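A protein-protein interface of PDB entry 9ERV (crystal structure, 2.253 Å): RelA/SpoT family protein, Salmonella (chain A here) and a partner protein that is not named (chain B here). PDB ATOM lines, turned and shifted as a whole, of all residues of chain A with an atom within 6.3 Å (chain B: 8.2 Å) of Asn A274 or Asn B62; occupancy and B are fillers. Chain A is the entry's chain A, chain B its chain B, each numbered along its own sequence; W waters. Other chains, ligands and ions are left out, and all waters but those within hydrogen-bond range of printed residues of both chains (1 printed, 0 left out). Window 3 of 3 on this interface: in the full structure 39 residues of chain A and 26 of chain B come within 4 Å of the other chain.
Among the printed residues, pairs that only touch across the chains: Ser A278 with Asn B62, Leu A275 with Asn B62, Asn A274 with Asn B62, Val A309 with Trp B65, Leu A275 with Trp B65 and Asp A272 with Trp B65.
NE2 of Gln B59 lies within hydrogen-bond range of O of Asn B62, at 3.4 Å. The side-chain amide nitrogen (NE2) of Gln B59 lies close to the backbone carbonyl oxygen (O) of Thr B61 (3.5 Å). The backbone carbonyl oxygen (O) of Asn A274 lies within hydrogen-bond range of the side-chain hydroxyl (OG) of Ser A278 (2.7 Å). The side-chain carboxylate of Asp A272 sits at hydrogen-bond distance from the backbone NH of Asn A274 (3.2 Å). The side-chain amide oxygen (OD1) of Asn A274 lies within hydrogen-bond range of the side-chain amino group (NZ) of Lys A277, at 3.4 Å. The backbone carbonyl oxygen (O) of Leu A275 is in hydrogen-bond range of the side-chain hydroxyl (OG) of Ser A278 (2.8 Å).
Printed residues of chain A that touch a printed residue of chain B: Asp A272, Asn A274, Leu A275, Ser A278 and Val A309. Hydrophobic or aromatic side chains of chain A within 4 Å of the printed part of chain B: Leu A275 and Val A309. Of the 8 printed residues of chain B, 4 touch a printed residue of chain A. Hydrophobic or aromatic side chains of chain B that line the printed part of chain A: Trp B65.
N of Val A309 is in hydrogen-bond range of O of Thr B63, 3.0 Å away. The side-chain amide nitrogen of Asn A274 is in hydrogen-bond range of the side-chain amide oxygen of Gln B59. OD2 of Asp A272 sits at hydrogen-bond distance from NE2 of Gln B59 (2.9 Å).
Asn A274 touches just these residues of chain B: Gln B59 and Asn B62. Of chain A, only Asn A274, Leu A275 and Ser A278 come within 4 Å of Asn B62. Of the printed residues of chain A, Trp B65 touches Asp A272, Leu A275 and Val A309. Printed residues of chain B within 4 Å of Asp A272: Gln B59 (2.9 Å) and Trp B65 (3.9 Å). Of the printed residues of chain B, Val A309 touches Thr B63 and Trp B65. Of the printed residues of chain A, Gln B59 touches Asp A272 (2.9 Å) and Asn A274 (2.9 Å). Of the printed residues of chain B, Ser A278 touches Asn B62 (2.8 Å). Lys A276 touches none of the printed residues of chain B. The nearest residue of chain B that does not touch Asn A274 is Thr B61 (5.6 Å). The nearest printed residue of chain B that does not touch Val A309 is Leu B64 (5.2 Å).
Water W1 lies within hydrogen-bond range of OD1 of Asp A272 (2.7 Å), NE1 of Trp B65 (3.1 Å) and OE1 of Gln B59 (3.2 Å).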
ATOM      1  N   ASP A 272      -5.483   0.356  19.403  1.00  0.00           N
ATOM      2  CA  ASP A 272      -4.154   0.381  19.989  1.00  0.00           C
ATOM      3  C   ASP A 272      -3.523   1.773  19.809  1.00  0.00           C
ATOM      4  O   ASP A 272      -3.714   2.402  18.765  1.00  0.00           O
ATOM      5  CB  ASP A 272      -3.284  -0.709  19.343  1.00  0.00           C
ATOM      6  CG  ASP A 272      -1.923  -0.830  19.972  1.00  0.00           C
ATOM      7  OD1 ASP A 272      -1.834  -1.397  21.091  1.00  0.00           O
ATOM      8  OD2 ASP A 272      -0.940  -0.353  19.354  1.00  0.00           O
ATOM      9  N   ALA A 273      -2.805   2.267  20.827  1.00  0.00           N
ATOM     10  CA  ALA A 273      -2.184   3.594  20.753  1.00  0.00           C
ATOM     11  C   ALA A 273      -1.054   3.697  19.718  1.00  0.00           C
ATOM     12  O   ALA A 273      -1.006   4.672  18.975  1.00  0.00           O
ATOM     13  CB  ALA A 273      -1.681   4.016  22.129  1.00  0.00           C
ATOM     14  N   ASN A 274      -0.158   2.694  19.661  1.00  0.00           N
ATOM     15  CA  ASN A 274       0.960   2.682  18.717  1.00  0.00           C
ATOM     16  C   ASN A 274       0.481   2.614  17.284  1.00  0.00           C
ATOM     17  O   ASN A 274       1.039   3.279  16.415  1.00  0.00           O
ATOM     18  CB  ASN A 274       1.907   1.525  19.003  1.00  0.00           C
ATOM     19  CG  ASN A 274       2.670   1.677  20.292  1.00  0.00           C
ATOM     20  OD1 ASN A 274       2.765   2.768  20.862  1.00  0.00           O
ATOM     21  ND2 ASN A 274       3.230   0.578  20.785  1.00  0.00           N
ATOM     22  N   LEU A 275      -0.565   1.826  17.031  1.00  0.00           N
ATOM     23  CA  LEU A 275      -1.139   1.688  15.703  1.00  0.00           C
ATOM     24  C   LEU A 275      -1.631   3.031  15.178  1.00  0.00           C
ATOM     25  O   LEU A 275      -1.403   3.360  14.018  1.00  0.00           O
ATOM     26  CB  LEU A 275      -2.302   0.692  15.771  1.00  0.00           C
ATOM     27  CG  LEU A 275      -3.056   0.459  14.481  1.00  0.00           C
ATOM     28  CD1 LEU A 275      -3.311  -0.990  14.293  1.00  0.00           C
ATOM     29  CD2 LEU A 275      -4.358   1.242  14.452  1.00  0.00           C
ATOM     30  N   LYS A 276      -2.298   3.802  16.043  1.00  0.00           N
ATOM     31  CA  LYS A 276      -2.868   5.099  15.713  1.00  0.00           C
ATOM     32  C   LYS A 276      -1.820   6.168  15.351  1.00  0.00           C
ATOM     33  O   LYS A 276      -2.122   7.050  14.546  1.00  0.00           O
ATOM     34  CB  LYS A 276      -3.795   5.577  16.831  1.00  0.00           C
ATOM     35  CG  LYS A 276      -5.064   4.749  16.955  1.00  0.00           C
ATOM     36  CD  LYS A 276      -5.802   5.110  18.229  1.00  0.00           C
ATOM     37  CE  LYS A 276      -7.160   4.474  18.306  1.00  0.00           C
ATOM     38  NZ  LYS A 276      -7.899   4.909  19.522  1.00  0.00           N
ATOM     39  N   LYS A 277      -0.588   6.078  15.841  1.00  0.00           N
ATOM     40  CA  LYS A 277       0.438   7.064  15.395  1.00  0.00           C
ATOM     41  C   LYS A 277       0.980   6.647  14.021  1.00  0.00           C
ATOM     42  O   LYS A 277       1.325   7.542  13.243  1.00  0.00           O
ATOM     43  CB  LYS A 277       1.533   7.212  16.457  1.00  0.00           C
ATOM     44  CG  LYS A 277       1.147   6.765  17.860  1.00  0.00           C
ATOM     45  CD  LYS A 277       2.334   6.424  18.734  1.00  0.00           C
ATOM     46  CE  LYS A 277       3.312   5.479  18.068  1.00  0.00           C
ATOM     47  NZ  LYS A 277       4.407   5.085  18.986  1.00  0.00           N
ATOM     48  N   SER A 278       0.997   5.355  13.718  1.00  0.00           N
ATOM     49  CA  SER A 278       1.433   4.806  12.406  1.00  0.00           C
ATOM     50  C   SER A 278       0.486   5.286  11.310  1.00  0.00           C
ATOM     51  O   SER A 278       0.873   5.240  10.143  1.00  0.00           O
ATOM     52  CB  SER A 278       1.489   3.314  12.416  1.00  0.00           C
ATOM     53  OG  SER A 278       1.304   2.817  13.725  1.00  0.00           O
ATOM     54  N   LEU A 279      -0.747   5.597  11.663  1.00  0.00           N
ATOM     55  CA  LEU A 279      -1.787   5.941  10.667  1.00  0.00           C
ATOM     56  C   LEU A 279      -1.450   7.258   9.975  1.00  0.00           C
ATOM     57  O   LEU A 279      -0.699   8.064  10.543  1.00  0.00           O
ATOM     58  CB  LEU A 279      -3.134   6.038  11.383  1.00  0.00           C
ATOM     59  CG  LEU A 279      -3.779   4.693  11.699  1.00  0.00           C
ATOM     60  CD1 LEU A 279      -5.029   4.875  12.539  1.00  0.00           C
ATOM     61  CD2 LEU A 279      -4.100   3.955  10.417  1.00  0.00           C
ATOM     62  N   VAL A 309      -2.177  -5.439  11.224  1.00  0.00           N
ATOM     63  CA  VAL A 309      -3.277  -4.552  10.867  1.00  0.00           C
ATOM     64  C   VAL A 309      -2.687  -3.606   9.860  1.00  0.00           C
ATOM     65  O   VAL A 309      -1.786  -2.861  10.202  1.00  0.00           O
ATOM     66  CB  VAL A 309      -3.886  -3.776  12.053  1.00  0.00           C
ATOM     67  CG1 VAL A 309      -4.925  -2.800  11.554  1.00  0.00           C
ATOM     68  CG2 VAL A 309      -4.494  -4.713  13.086  1.00  0.00           C
ATOM     69  N   MET B  46      -2.348  -8.325  27.691  1.00  0.00           N
ATOM     70  CA  MET B  46      -1.525  -8.812  26.592  1.00  0.00           C
ATOM     71  C   MET B  46      -1.675 -10.317  26.454  1.00  0.00           C
ATOM     72  O   MET B  46      -0.686 -11.051  26.432  1.00  0.00           O
ATOM     73  CB  MET B  46      -0.074  -8.336  26.699  1.00  0.00           C
ATOM     74  CG  MET B  46       0.084  -6.844  26.437  1.00  0.00           C
ATOM     75  SD  MET B  46      -0.274  -6.302  24.730  1.00  0.00           S
ATOM     76  CE  MET B  46       1.307  -6.558  23.964  1.00  0.00           C
ATOM     77  N   GLN B  59       3.910  -6.879  20.991  1.00  0.00           N
ATOM     78  CA  GLN B  59       3.886  -5.999  19.831  1.00  0.00           C
ATOM     79  C   GLN B  59       5.276  -5.929  19.263  1.00  0.00           C
ATOM     80  O   GLN B  59       6.195  -5.539  19.976  1.00  0.00           O
ATOM     81  CB  GLN B  59       3.424  -4.593  20.212  1.00  0.00           C
ATOM     82  CG  GLN B  59       2.764  -3.858  19.045  1.00  0.00           C
ATOM     83  CD  GLN B  59       2.050  -2.598  19.455  1.00  0.00           C
ATOM     84  OE1 GLN B  59       2.186  -2.110  20.584  1.00  0.00           O
ATOM     85  NE2 GLN B  59       1.274  -2.036  18.542  1.00  0.00           N
ATOM     86  N   LEU B  60       5.449  -6.310  17.993  1.00  0.00           N
ATOM     87  CA  LEU B  60       6.756  -6.252  17.355  1.00  0.00           C
ATOM     88  C   LEU B  60       6.946  -4.881  16.702  1.00  0.00           C
ATOM     89  O   LEU B  60       7.996  -4.278  16.853  1.00  0.00           O
ATOM     90  CB  LEU B  60       6.918  -7.392  16.332  1.00  0.00           C
ATOM     91  CG  LEU B  60       6.592  -8.809  16.829  1.00  0.00           C
ATOM     92  CD1 LEU B  60       6.851  -9.838  15.731  1.00  0.00           C
ATOM     93  CD2 LEU B  60       7.391  -9.170  18.082  1.00  0.00           C
ATOM     94  N   THR B  61       5.934  -4.397  15.972  1.00  0.00           N
ATOM     95  CA  THR B  61       5.906  -3.075  15.325  1.00  0.00           C
ATOM     96  C   THR B  61       4.521  -2.389  15.606  1.00  0.00           C
ATOM     97  O   THR B  61       3.646  -3.006  16.215  1.00  0.00           O
ATOM     98  CB  THR B  61       6.263  -3.163  13.805  1.00  0.00           C
ATOM     99  OG1 THR B  61       5.133  -3.583  13.047  1.00  0.00           O
ATOM    100  CG2 THR B  61       7.422  -4.068  13.511  1.00  0.00           C
ATOM    101  N   ASN B  62       4.307  -1.135  15.166  1.00  0.00           N
ATOM    102  CA  ASN B  62       3.030  -0.429  15.394  1.00  0.00           C
ATOM    103  C   ASN B  62       1.813  -1.174  14.834  1.00  0.00           C
ATOM    104  O   ASN B  62       0.711  -1.042  15.349  1.00  0.00           O
ATOM    105  CB  ASN B  62       3.073   0.960  14.770  1.00  0.00           C
ATOM    106  CG  ASN B  62       4.079   1.866  15.402  1.00  0.00           C
ATOM    107  OD1 ASN B  62       4.290   1.835  16.618  1.00  0.00           O
ATOM    108  ND2 ASN B  62       4.711   2.711  14.599  1.00  0.00           N
ATOM    109  N   THR B  63       2.025  -1.957  13.780  1.00  0.00           N
ATOM    110  CA  THR B  63       0.991  -2.689  13.089  1.00  0.00           C
ATOM    111  C   THR B  63       1.203  -4.214  13.134  1.00  0.00           C
ATOM    112  O   THR B  63       0.537  -4.917  12.377  1.00  0.00           O
ATOM    113  CB  THR B  63       0.973  -2.198  11.631  1.00  0.00           C
ATOM    114  OG1 THR B  63       2.271  -2.357  11.047  1.00  0.00           O
ATOM    115  CG2 THR B  63       0.562  -0.733  11.512  1.00  0.00           C
ATOM    116  N   LEU B  64       2.116  -4.733  13.986  1.00  0.00           N
ATOM    117  CA  LEU B  64       2.384  -6.173  14.011  1.00  0.00           C
ATOM    118  C   LEU B  64       2.523  -6.762  15.421  1.00  0.00           C
ATOM    119  O   LEU B  64       3.153  -6.167  16.276  1.00  0.00           O
ATOM    120  CB  LEU B  64       3.614  -6.486  13.150  1.00  0.00           C
ATOM    121  CG  LEU B  64       4.016  -7.959  13.006  1.00  0.00           C
ATOM    122  CD1 LEU B  64       3.101  -8.695  12.028  1.00  0.00           C
ATOM    123  CD2 LEU B  64       5.478  -8.083  12.613  1.00  0.00           C
ATOM    124  N   TRP B  65       1.917  -7.931  15.654  1.00  0.00           N
ATOM    125  CA  TRP B  65       1.920  -8.645  16.934  1.00  0.00           C
ATOM    126  C   TRP B  65       2.235 -10.119  16.741  1.00  0.00           C
ATOM    127  O   TRP B  65       1.924 -10.681  15.709  1.00  0.00           O
ATOM    128  CB  TRP B  65       0.522  -8.585  17.599  1.00  0.00           C
ATOM    129  CG  TRP B  65       0.101  -7.231  18.055  1.00  0.00           C
ATOM    130  CD1 TRP B  65       0.254  -6.703  19.300  1.00  0.00           C
ATOM    131  CD2 TRP B  65      -0.583  -6.241  17.278  1.00  0.00           C
ATOM    132  NE1 TRP B  65      -0.319  -5.459  19.356  1.00  0.00           N
ATOM    133  CE2 TRP B  65      -0.807  -5.134  18.116  1.00  0.00           C
ATOM    134  CE3 TRP B  65      -1.023  -6.182  15.951  1.00  0.00           C
ATOM    135  CZ2 TRP B  65      -1.442  -3.974  17.669  1.00  0.00           C
ATOM    136  CZ3 TRP B  65      -1.610  -5.017  15.496  1.00  0.00           C
ATOM    137  CH2 TRP B  65      -1.820  -3.928  16.352  1.00  0.00           C
HETATM  138  O   HOH W   1      -0.413  -3.549  21.844  1.00  0.00           O
